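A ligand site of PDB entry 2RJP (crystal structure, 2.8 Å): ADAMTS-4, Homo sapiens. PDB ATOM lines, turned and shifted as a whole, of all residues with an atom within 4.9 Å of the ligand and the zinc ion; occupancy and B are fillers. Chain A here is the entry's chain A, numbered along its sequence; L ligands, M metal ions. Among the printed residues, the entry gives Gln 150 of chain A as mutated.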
ATOM      1  N   ALA A  36     -34.580 -11.582 -21.908  1.00  0.00           N
ATOM      2  CA  ALA A  36     -34.430 -10.131 -21.892  1.00  0.00           C
ATOM      3  C   ALA A  36     -33.173  -9.705 -22.647  1.00  0.00           C
ATOM      4  O   ALA A  36     -33.232  -8.808 -23.481  1.00  0.00           O
ATOM      5  CB  ALA A  36     -34.406  -9.614 -20.470  1.00  0.00           C
ATOM      6  N   ALA A  40     -32.900  -7.280 -26.257  1.00  0.00           N
ATOM      7  CA  ALA A  40     -32.076  -6.105 -26.515  1.00  0.00           C
ATOM      8  C   ALA A  40     -31.367  -6.230 -27.869  1.00  0.00           C
ATOM      9  O   ALA A  40     -31.279  -5.251 -28.611  1.00  0.00           O
ATOM     10  CB  ALA A  40     -31.072  -5.870 -25.382  1.00  0.00           C
ATOM     11  N   ASP A 116     -17.947  -2.153  -7.414  1.00  0.00           N
ATOM     12  CA  ASP A 116     -19.099  -1.757  -8.251  1.00  0.00           C
ATOM     13  C   ASP A 116     -19.118  -2.489  -9.599  1.00  0.00           C
ATOM     14  O   ASP A 116     -20.146  -2.502 -10.280  1.00  0.00           O
ATOM     15  CB  ASP A 116     -19.107  -0.239  -8.467  1.00  0.00           C
ATOM     16  CG  ASP A 116     -19.221   0.554  -7.156  1.00  0.00           C
ATOM     17  OD1 ASP A 116     -19.913   0.084  -6.225  1.00  0.00           O
ATOM     18  OD2 ASP A 116     -18.624   1.643  -7.062  1.00  0.00           O
ATOM     19  N   THR A 117     -17.992  -3.081  -9.973  1.00  0.00           N
ATOM     20  CA  THR A 117     -17.921  -3.956 -11.148  1.00  0.00           C
ATOM     21  C   THR A 117     -19.067  -4.969 -11.146  1.00  0.00           C
ATOM     22  O   THR A 117     -19.314  -5.624 -10.128  1.00  0.00           O
ATOM     23  CB  THR A 117     -16.568  -4.694 -11.184  1.00  0.00           C
ATOM     24  OG1 THR A 117     -15.511  -3.742 -11.240  1.00  0.00           O
ATOM     25  CG2 THR A 117     -16.468  -5.635 -12.376  1.00  0.00           C
ATOM     26  N   LEU A 118     -19.767  -5.078 -12.269  1.00  0.00           N
ATOM     27  CA  LEU A 118     -20.898  -6.007 -12.382  1.00  0.00           C
ATOM     28  C   LEU A 118     -20.663  -7.161 -13.369  1.00  0.00           C
ATOM     29  O   LEU A 118     -21.454  -8.099 -13.417  1.00  0.00           O
ATOM     30  CB  LEU A 118     -22.195  -5.260 -12.693  1.00  0.00           C
ATOM     31  CG  LEU A 118     -22.823  -4.510 -11.503  1.00  0.00           C
ATOM     32  CD1 LEU A 118     -23.986  -3.654 -11.930  1.00  0.00           C
ATOM     33  CD2 LEU A 118     -23.264  -5.473 -10.406  1.00  0.00           C
ATOM     34  N   GLY A 119     -19.588  -7.087 -14.143  1.00  0.00           N
ATOM     35  CA  GLY A 119     -19.266  -8.155 -15.084  1.00  0.00           C
ATOM     36  C   GLY A 119     -18.027  -7.868 -15.906  1.00  0.00           C
ATOM     37  O   GLY A 119     -17.470  -6.787 -15.829  1.00  0.00           O
ATOM     38  N   MET A 120     -17.610  -8.844 -16.698  1.00  0.00           N
ATOM     39  CA  MET A 120     -16.364  -8.708 -17.459  1.00  0.00           C
ATOM     40  C   MET A 120     -16.365  -9.582 -18.708  1.00  0.00           C
ATOM     41  O   MET A 120     -16.882 -10.689 -18.706  1.00  0.00           O
ATOM     42  CB  MET A 120     -15.154  -9.035 -16.569  1.00  0.00           C
ATOM     43  CG  MET A 120     -13.848  -8.492 -17.093  1.00  0.00           C
ATOM     44  SD  MET A 120     -12.486  -8.591 -15.915  1.00  0.00           S
ATOM     45  CE  MET A 120     -12.269  -6.889 -15.428  1.00  0.00           C
ATOM     46  N   PHE A 145     -29.400  -6.898 -18.333  1.00  0.00           N
ATOM     47  CA  PHE A 145     -28.759  -5.719 -18.896  1.00  0.00           C
ATOM     48  C   PHE A 145     -27.240  -5.823 -18.842  1.00  0.00           C
ATOM     49  O   PHE A 145     -26.556  -5.422 -19.784  1.00  0.00           O
ATOM     50  CB  PHE A 145     -29.260  -4.466 -18.183  1.00  0.00           C
ATOM     51  CG  PHE A 145     -30.770  -4.344 -18.187  1.00  0.00           C
ATOM     52  CD1 PHE A 145     -31.551  -5.056 -19.099  1.00  0.00           C
ATOM     53  CD2 PHE A 145     -31.407  -3.485 -17.294  1.00  0.00           C
ATOM     54  CE1 PHE A 145     -32.948  -4.938 -19.111  1.00  0.00           C
ATOM     55  CE2 PHE A 145     -32.805  -3.359 -17.296  1.00  0.00           C
ATOM     56  CZ  PHE A 145     -33.578  -4.074 -18.204  1.00  0.00           C
ATOM     57  N   THR A 146     -26.698  -6.362 -17.753  1.00  0.00           N
ATOM     58  CA  THR A 146     -25.253  -6.547 -17.630  1.00  0.00           C
ATOM     59  C   THR A 146     -24.793  -7.523 -18.709  1.00  0.00           C
ATOM     60  O   THR A 146     -23.745  -7.327 -19.339  1.00  0.00           O
ATOM     61  CB  THR A 146     -24.865  -7.065 -16.232  1.00  0.00           C
ATOM     62  OG1 THR A 146     -25.582  -6.336 -15.235  1.00  0.00           O
ATOM     63  CG2 THR A 146     -23.374  -6.920 -15.986  1.00  0.00           C
ATOM     64  N   ALA A 148     -26.350  -8.247 -21.700  1.00  0.00           N
ATOM     65  CA  ALA A 148     -26.413  -7.600 -23.023  1.00  0.00           C
ATOM     66  C   ALA A 148     -25.191  -6.732 -23.261  1.00  0.00           C
ATOM     67  O   ALA A 148     -24.644  -6.684 -24.368  1.00  0.00           O
ATOM     68  CB  ALA A 148     -27.685  -6.763 -23.149  1.00  0.00           C
ATOM     69  N   HIS A 149     -24.755  -6.032 -22.211  1.00  0.00           N
ATOM     70  CA  HIS A 149     -23.566  -5.195 -22.270  1.00  0.00           C
ATOM     71  C   HIS A 149     -22.320  -6.053 -22.506  1.00  0.00           C
ATOM     72  O   HIS A 149     -21.505  -5.752 -23.373  1.00  0.00           O
ATOM     73  CB  HIS A 149     -23.447  -4.380 -20.969  1.00  0.00           C
ATOM     74  CG  HIS A 149     -22.216  -3.535 -20.868  1.00  0.00           C
ATOM     75  ND1 HIS A 149     -22.228  -2.182 -21.094  1.00  0.00           N
ATOM     76  CD2 HIS A 149     -20.942  -3.848 -20.548  1.00  0.00           C
ATOM     77  CE1 HIS A 149     -21.013  -1.695 -20.922  1.00  0.00           C
ATOM     78  NE2 HIS A 149     -20.216  -2.687 -20.587  1.00  0.00           N
ATOM     79  N   GLN A 150     -22.208  -7.147 -21.739  1.00  0.00           N
ATOM     80  CA  GLN A 150     -21.061  -8.041 -21.802  1.00  0.00           C
ATOM     81  C   GLN A 150     -20.926  -8.714 -23.156  1.00  0.00           C
ATOM     82  O   GLN A 150     -19.812  -8.851 -23.677  1.00  0.00           O
ATOM     83  CB  GLN A 150     -21.098  -9.080 -20.687  1.00  0.00           C
ATOM     84  CG  GLN A 150     -20.935  -8.530 -19.279  1.00  0.00           C
ATOM     85  CD  GLN A 150     -19.705  -7.637 -19.107  1.00  0.00           C
ATOM     86  OE1 GLN A 150     -18.698  -7.809 -19.787  1.00  0.00           O
ATOM     87  NE2 GLN A 150     -19.790  -6.684 -18.180  1.00  0.00           N
ATOM     88  N   HIS A 153     -19.512  -6.254 -25.632  1.00  0.00           N
ATOM     89  CA  HIS A 153     -18.063  -6.347 -25.649  1.00  0.00           C
ATOM     90  C   HIS A 153     -17.599  -7.553 -26.492  1.00  0.00           C
ATOM     91  O   HIS A 153     -16.740  -7.407 -27.370  1.00  0.00           O
ATOM     92  CB  HIS A 153     -17.489  -6.452 -24.223  1.00  0.00           C
ATOM     93  CG  HIS A 153     -17.425  -5.147 -23.486  1.00  0.00           C
ATOM     94  ND1 HIS A 153     -16.759  -4.043 -23.971  1.00  0.00           N
ATOM     95  CD2 HIS A 153     -17.897  -4.786 -22.266  1.00  0.00           C
ATOM     96  CE1 HIS A 153     -16.848  -3.057 -23.096  1.00  0.00           C
ATOM     97  NE2 HIS A 153     -17.531  -3.478 -22.057  1.00  0.00           N
ATOM     98  N   HIS A 159     -16.965   1.108 -25.060  1.00  0.00           N
ATOM     99  CA  HIS A 159     -17.858   1.982 -24.304  1.00  0.00           C
ATOM    100  C   HIS A 159     -18.189   3.272 -25.064  1.00  0.00           C
ATOM    101  O   HIS A 159     -17.437   3.675 -25.945  1.00  0.00           O
ATOM    102  CB  HIS A 159     -17.243   2.321 -22.940  1.00  0.00           C
ATOM    103  CG  HIS A 159     -17.290   1.197 -21.959  1.00  0.00           C
ATOM    104  ND1 HIS A 159     -16.389   1.080 -20.932  1.00  0.00           N
ATOM    105  CD2 HIS A 159     -18.109   0.129 -21.860  1.00  0.00           C
ATOM    106  CE1 HIS A 159     -16.662   0.005 -20.225  1.00  0.00           C
ATOM    107  NE2 HIS A 159     -17.707  -0.600 -20.765  1.00  0.00           N
ATOM    108  N   HIS A 177     -27.453   4.447 -23.273  1.00  0.00           N
ATOM    109  CA  HIS A 177     -27.265   3.303 -24.158  1.00  0.00           C
ATOM    110  C   HIS A 177     -26.620   2.125 -23.429  1.00  0.00           C
ATOM    111  O   HIS A 177     -25.995   2.312 -22.394  1.00  0.00           O
ATOM    112  CB  HIS A 177     -26.442   3.700 -25.381  1.00  0.00           C
ATOM    113  CG  HIS A 177     -26.915   4.939 -26.042  1.00  0.00           C
ATOM    114  ND1 HIS A 177     -28.089   5.004 -26.775  1.00  0.00           N
ATOM    115  CD2 HIS A 177     -26.395   6.190 -26.080  1.00  0.00           C
ATOM    116  CE1 HIS A 177     -28.259   6.221 -27.225  1.00  0.00           C
ATOM    117  NE2 HIS A 177     -27.250   6.970 -26.824  1.00  0.00           N
ATOM    118  N   VAL A 178     -26.771   0.928 -23.994  1.00  0.00           N
ATOM    119  CA  VAL A 178     -26.241  -0.306 -23.417  1.00  0.00           C
ATOM    120  C   VAL A 178     -24.739  -0.229 -23.109  1.00  0.00           C
ATOM    121  O   VAL A 178     -24.295  -0.697 -22.053  1.00  0.00           O
ATOM    122  CB  VAL A 178     -26.546  -1.527 -24.332  1.00  0.00           C
ATOM    123  CG1 VAL A 178     -25.965  -2.806 -23.751  1.00  0.00           C
ATOM    124  CG2 VAL A 178     -28.045  -1.689 -24.541  1.00  0.00           C
ATOM    125  N   MET A 179     -23.980   0.378 -24.018  1.00  0.00           N
ATOM    126  CA  MET A 179     -22.521   0.387 -23.888  1.00  0.00           C
ATOM    127  C   MET A 179     -21.946   1.601 -23.133  1.00  0.00           C
ATOM    128  O   MET A 179     -20.793   1.983 -23.327  1.00  0.00           O
ATOM    129  CB  MET A 179     -21.847   0.146 -25.248  1.00  0.00           C
ATOM    130  CG  MET A 179     -22.190  -1.212 -25.879  1.00  0.00           C
ATOM    131  SD  MET A 179     -22.035  -2.659 -24.787  1.00  0.00           S
ATOM    132  CE  MET A 179     -20.252  -2.825 -24.629  1.00  0.00           C
ATOM    133  N   ALA A 180     -22.775   2.174 -22.267  1.00  0.00           N
ATOM    134  CA  ALA A 180     -22.354   3.204 -21.316  1.00  0.00           C
ATOM    135  C   ALA A 180     -21.310   2.608 -20.362  1.00  0.00           C
ATOM    136  O   ALA A 180     -21.379   1.428 -20.073  1.00  0.00           O
ATOM    137  CB  ALA A 180     -23.549   3.704 -20.545  1.00  0.00           C
ATOM    138  N   PRO A 181     -20.341   3.414 -19.895  1.00  0.00           N
ATOM    139  CA  PRO A 181     -19.309   2.854 -18.997  1.00  0.00           C
ATOM    140  C   PRO A 181     -19.841   2.471 -17.618  1.00  0.00           C
ATOM    141  O   PRO A 181     -19.249   1.631 -16.937  1.00  0.00           O
ATOM    142  CB  PRO A 181     -18.291   3.989 -18.885  1.00  0.00           C
ATOM    143  CG  PRO A 181     -19.059   5.223 -19.157  1.00  0.00           C
ATOM    144  CD  PRO A 181     -20.122   4.857 -20.156  1.00  0.00           C
ATOM    145  N   VAL A 182     -20.949   3.093 -17.211  1.00  0.00           N
ATOM    146  CA  VAL A 182     -21.631   2.743 -15.968  1.00  0.00           C
ATOM    147  C   VAL A 182     -23.071   2.330 -16.247  1.00  0.00           C
ATOM    148  O   VAL A 182     -23.602   2.652 -17.313  1.00  0.00           O
ATOM    149  CB  VAL A 182     -21.643   3.909 -14.941  1.00  0.00           C
ATOM    150  CG1 VAL A 182     -20.230   4.222 -14.467  1.00  0.00           C
ATOM    151  CG2 VAL A 182     -22.353   5.147 -15.537  1.00  0.00           C
ATOM    152  N   MET A 183     -23.701   1.644 -15.304  1.00  0.00           N
ATOM    153  CA  MET A 183     -25.108   1.284 -15.421  1.00  0.00           C
ATOM    154  C   MET A 183     -25.924   2.525 -15.767  1.00  0.00           C
ATOM    155  O   MET A 183     -25.782   3.571 -15.127  1.00  0.00           O
ATOM    156  CB  MET A 183     -25.610   0.650 -14.126  1.00  0.00           C
ATOM    157  CG  MET A 183     -27.045   0.104 -14.178  1.00  0.00           C
ATOM    158  SD  MET A 183     -27.187  -1.459 -15.098  1.00  0.00           S
ATOM    159  CE  MET A 183     -28.783  -2.073 -14.518  1.00  0.00           C
ATOM    160  N   ALA A 184     -26.752   2.414 -16.791  1.00  0.00           N
ATOM    161  CA  ALA A 184     -27.518   3.546 -17.271  1.00  0.00           C
ATOM    162  C   ALA A 184     -28.956   3.143 -17.547  1.00  0.00           C
ATOM    163  O   ALA A 184     -29.226   1.988 -17.884  1.00  0.00           O
ATOM    164  CB  ALA A 184     -26.893   4.090 -18.526  1.00  0.00           C
ATOM    165  N   VAL A 186     -31.561   2.863 -20.051  1.00  0.00           N
ATOM    166  CA  VAL A 186     -31.403   2.792 -21.497  1.00  0.00           C
ATOM    167  C   VAL A 186     -32.660   3.196 -22.257  1.00  0.00           C
ATOM    168  O   VAL A 186     -33.768   2.835 -21.868  1.00  0.00           O
ATOM    169  CB  VAL A 186     -30.932   1.399 -21.924  1.00  0.00           C
ATOM    170  CG1 VAL A 186     -30.629   1.372 -23.392  1.00  0.00           C
ATOM    171  CG2 VAL A 186     -29.710   1.042 -21.151  1.00  0.00           C
ATOM    172  N   ASP A 187     -32.458   3.948 -23.337  1.00  0.00           N
ATOM    173  CA  ASP A 187     -33.536   4.407 -24.201  1.00  0.00           C
ATOM    174  C   ASP A 187     -34.235   3.213 -24.819  1.00  0.00           C
ATOM    175  O   ASP A 187     -33.622   2.483 -25.599  1.00  0.00           O
ATOM    176  CB  ASP A 187     -32.966   5.309 -25.306  1.00  0.00           C
ATOM    177  CG  ASP A 187     -34.026   6.225 -25.924  1.00  0.00           C
ATOM    178  OD1 ASP A 187     -35.240   5.933 -25.789  1.00  0.00           O
ATOM    179  OD2 ASP A 187     -33.621   7.228 -26.540  1.00  0.00           O
ATOM    180  N   PRO A 188     -35.507   2.979 -24.451  1.00  0.00           N
ATOM    181  CA  PRO A 188     -36.228   1.868 -25.090  1.00  0.00           C
ATOM    182  C   PRO A 188     -36.383   2.063 -26.604  1.00  0.00           C
ATOM    183  O   PRO A 188     -36.416   1.066 -27.346  1.00  0.00           O
ATOM    184  CB  PRO A 188     -37.590   1.865 -24.384  1.00  0.00           C
ATOM    185  CG  PRO A 188     -37.722   3.207 -23.746  1.00  0.00           C
ATOM    186  CD  PRO A 188     -36.330   3.691 -23.457  1.00  0.00           C
ATOM    187  N   PRO A 191     -31.708   1.522 -27.737  1.00  0.00           N
ATOM    188  CA  PRO A 191     -30.785   0.995 -26.728  1.00  0.00           C
ATOM    189  C   PRO A 191     -29.333   1.044 -27.163  1.00  0.00           C
ATOM    190  O   PRO A 191     -28.443   1.169 -26.319  1.00  0.00           O
ATOM    191  CB  PRO A 191     -31.225  -0.476 -26.584  1.00  0.00           C
ATOM    192  CG  PRO A 191     -32.520  -0.589 -27.290  1.00  0.00           C
ATOM    193  CD  PRO A 191     -32.540   0.469 -28.328  1.00  0.00           C
ATOM    194  N   ASP A 279     -39.794  -4.487 -17.063  1.00  0.00           N
ATOM    195  CA  ASP A 279     -40.818  -4.341 -18.094  1.00  0.00           C
ATOM    196  C   ASP A 279     -41.998  -5.247 -17.822  1.00  0.00           C
ATOM    197  O   ASP A 279     -41.841  -6.461 -17.714  1.00  0.00           O
ATOM    198  CB  ASP A 279     -40.232  -4.697 -19.461  1.00  0.00           C
ATOM    199  CG  ASP A 279     -39.300  -3.632 -20.004  1.00  0.00           C
ATOM    200  OD1 ASP A 279     -39.077  -2.594 -19.319  1.00  0.00           O
ATOM    201  OD2 ASP A 279     -38.783  -3.845 -21.132  1.00  0.00           O
HETATM  202  C1  LIG L   1     -14.697  -3.856 -15.241  1.00  0.00           C
HETATM  203  C2  LIG L   1     -15.102  -3.705 -16.722  1.00  0.00           C
HETATM  204  C3  LIG L   1     -14.384  -4.801 -17.523  1.00  0.00           C
HETATM  205  C4  LIG L   1     -16.637  -3.749 -16.855  1.00  0.00           C
HETATM  206  C5  LIG L   1     -17.160  -3.572 -18.327  1.00  0.00           C
HETATM  207  O1  LIG L   1     -16.882  -2.447 -18.831  1.00  0.00           O
HETATM  208  O2  LIG L   1     -17.787  -4.521 -18.843  1.00  0.00           O
HETATM  209  N1  LIG L   1     -17.167  -2.534 -16.126  1.00  0.00           N
HETATM  210  S1  LIG L   1     -18.377  -2.762 -14.979  1.00  0.00           S
HETATM  211  O3  LIG L   1     -18.199  -1.706 -13.984  1.00  0.00           O
HETATM  212  O4  LIG L   1     -18.392  -4.149 -14.561  1.00  0.00           O
HETATM  213  C6  LIG L   1     -19.891  -2.471 -15.859  1.00  0.00           C
HETATM  214  C7  LIG L   1     -20.279  -1.158 -16.127  1.00  0.00           C
HETATM  215  C8  LIG L   1     -21.473  -0.930 -16.816  1.00  0.00           C
HETATM  216  C9  LIG L   1     -22.304  -1.998 -17.246  1.00  0.00           C
HETATM  217  C10 LIG L   1     -21.878  -3.312 -16.962  1.00  0.00           C
HETATM  218  C11 LIG L   1     -20.690  -3.550 -16.266  1.00  0.00           C
HETATM  219  C12 LIG L   1     -23.575  -1.726 -17.961  1.00  0.00           C
HETATM  220  C13 LIG L   1     -24.642  -2.651 -17.916  1.00  0.00           C
HETATM  221  C14 LIG L   1     -25.861  -2.402 -18.581  1.00  0.00           C
HETATM  222  C15 LIG L   1     -26.051  -1.208 -19.292  1.00  0.00           C
HETATM  223  C16 LIG L   1     -24.995  -0.271 -19.329  1.00  0.00           C
HETATM  224  C17 LIG L   1     -23.787  -0.527 -18.671  1.00  0.00           C
HETATM  225  C18 LIG L   1     -27.336  -0.906 -20.032  1.00  0.00           C
HETATM  226  O5  LIG L   1     -28.413  -1.737 -19.588  1.00  0.00           O
HETATM  227  C19 LIG L   1     -29.362  -2.281 -20.419  1.00  0.00           C
HETATM  228  C20 LIG L   1     -29.198  -3.219 -21.453  1.00  0.00           C
HETATM  229  C21 LIG L   1     -30.316  -3.683 -22.181  1.00  0.00           C
HETATM  230  C22 LIG L   1     -31.622  -3.240 -21.900  1.00  0.00           C
HETATM  231  C23 LIG L   1     -31.774  -2.318 -20.851  1.00  0.00           C
HETATM  232  C24 LIG L   1     -30.665  -1.852 -20.126  1.00  0.00           C
HETATM  233  C25 LIG L   1     -32.845  -3.739 -22.643  1.00  0.00           C
HETATM  234  O6  LIG L   1     -33.022  -4.955 -22.600  1.00  0.00           O
HETATM  235  C26 LIG L   1     -34.029  -2.863 -23.088  1.00  0.00           C
HETATM  236  C27 LIG L   1     -33.603  -1.583 -23.794  1.00  0.00           C
HETATM  237  C28 LIG L   1     -35.035  -2.609 -21.962  1.00  0.00           C
HETATM  238 ZN    ZN M   1     -18.169  -2.487 -20.320  1.00  0.00          ZN
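Ala 36 touches the ligand (O to O6, 3.96 Å).
CB of Ala 40 touches O6 of the ligand, 3.5 Å away.
CG2 of Thr 117 touches O4 of the ligand, at 3.3 Å.
CE of Met 120 touches C3 of the ligand, 3.6 Å away.
CB of Phe 145 touches C19 of the ligand (3.1 Å).
Thr 146 touches the ligand (CA to C13, 3.95 Å).
O of Val 178 touches C16 of the ligand (2.8 Å).
O of Ala 180 touches C17 of the ligand, 3.4 Å away.
Pro 181 touches the ligand.
Val 182 touches the ligand.
Met 183 touches the ligand (N to C8, 3.7 Å).
Val 186 touches the ligand.
Pro 191 touches the ligand (CG to C27, 3.8 Å).
Of the 27 residues printed, 19 come within 4 Å of the ligand.
Along chain A the residues within 4 Å of the ligand span positions 36 to 191.
Within 4 Å of the zinc ion: His 149, His 153 and His 159.
The nearest printed residue that does not touch the zinc ion is Met 179 (4.8 Å).
O2 of the ligand lies close to NE2 of Gln 150 (3.0 Å).
N of Leu 118 is in hydrogen-bond range of O4 of the ligand.
The backbone NH of Gly 119 is in hydrogen-bond range of an oxygen (O4) of the ligand (3.2 Å).
The zinc ion is bound by an oxygen (O1) of the ligand.
The zinc ion is bound by a ring nitrogen (NE2) of His 159 (2.0 Å).
NE2 of His 149 is bound to the zinc ion (2.1 Å).
NE2 of His 153 is bound to the zinc ion, at 2.1 Å.
The zinc ion is bound by O2 of the ligand.
The zinc ion has five donor atoms within binding distance.
The backbone carbonyl oxygen (O) of Gly 119 lies close to the side-chain amide nitrogen (NE2) of Gln 150 (3.3 Å).
A ring nitrogen (ND1) of His 149 lies within hydrogen-bond range of the backbone carbonyl oxygen (O) of Val 178, at 2.7 Å.
N of Val 178 lies within hydrogen-bond range of O of Pro 191 (2.9 Å).
A ring nitrogen (ND1) of His 149 lies within hydrogen-bond range of the side-chain sulfur (SD) of Met 179 (3.7 Å).
N of Met 120 sits close to NE2 of Gln 150 (3.4 Å).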
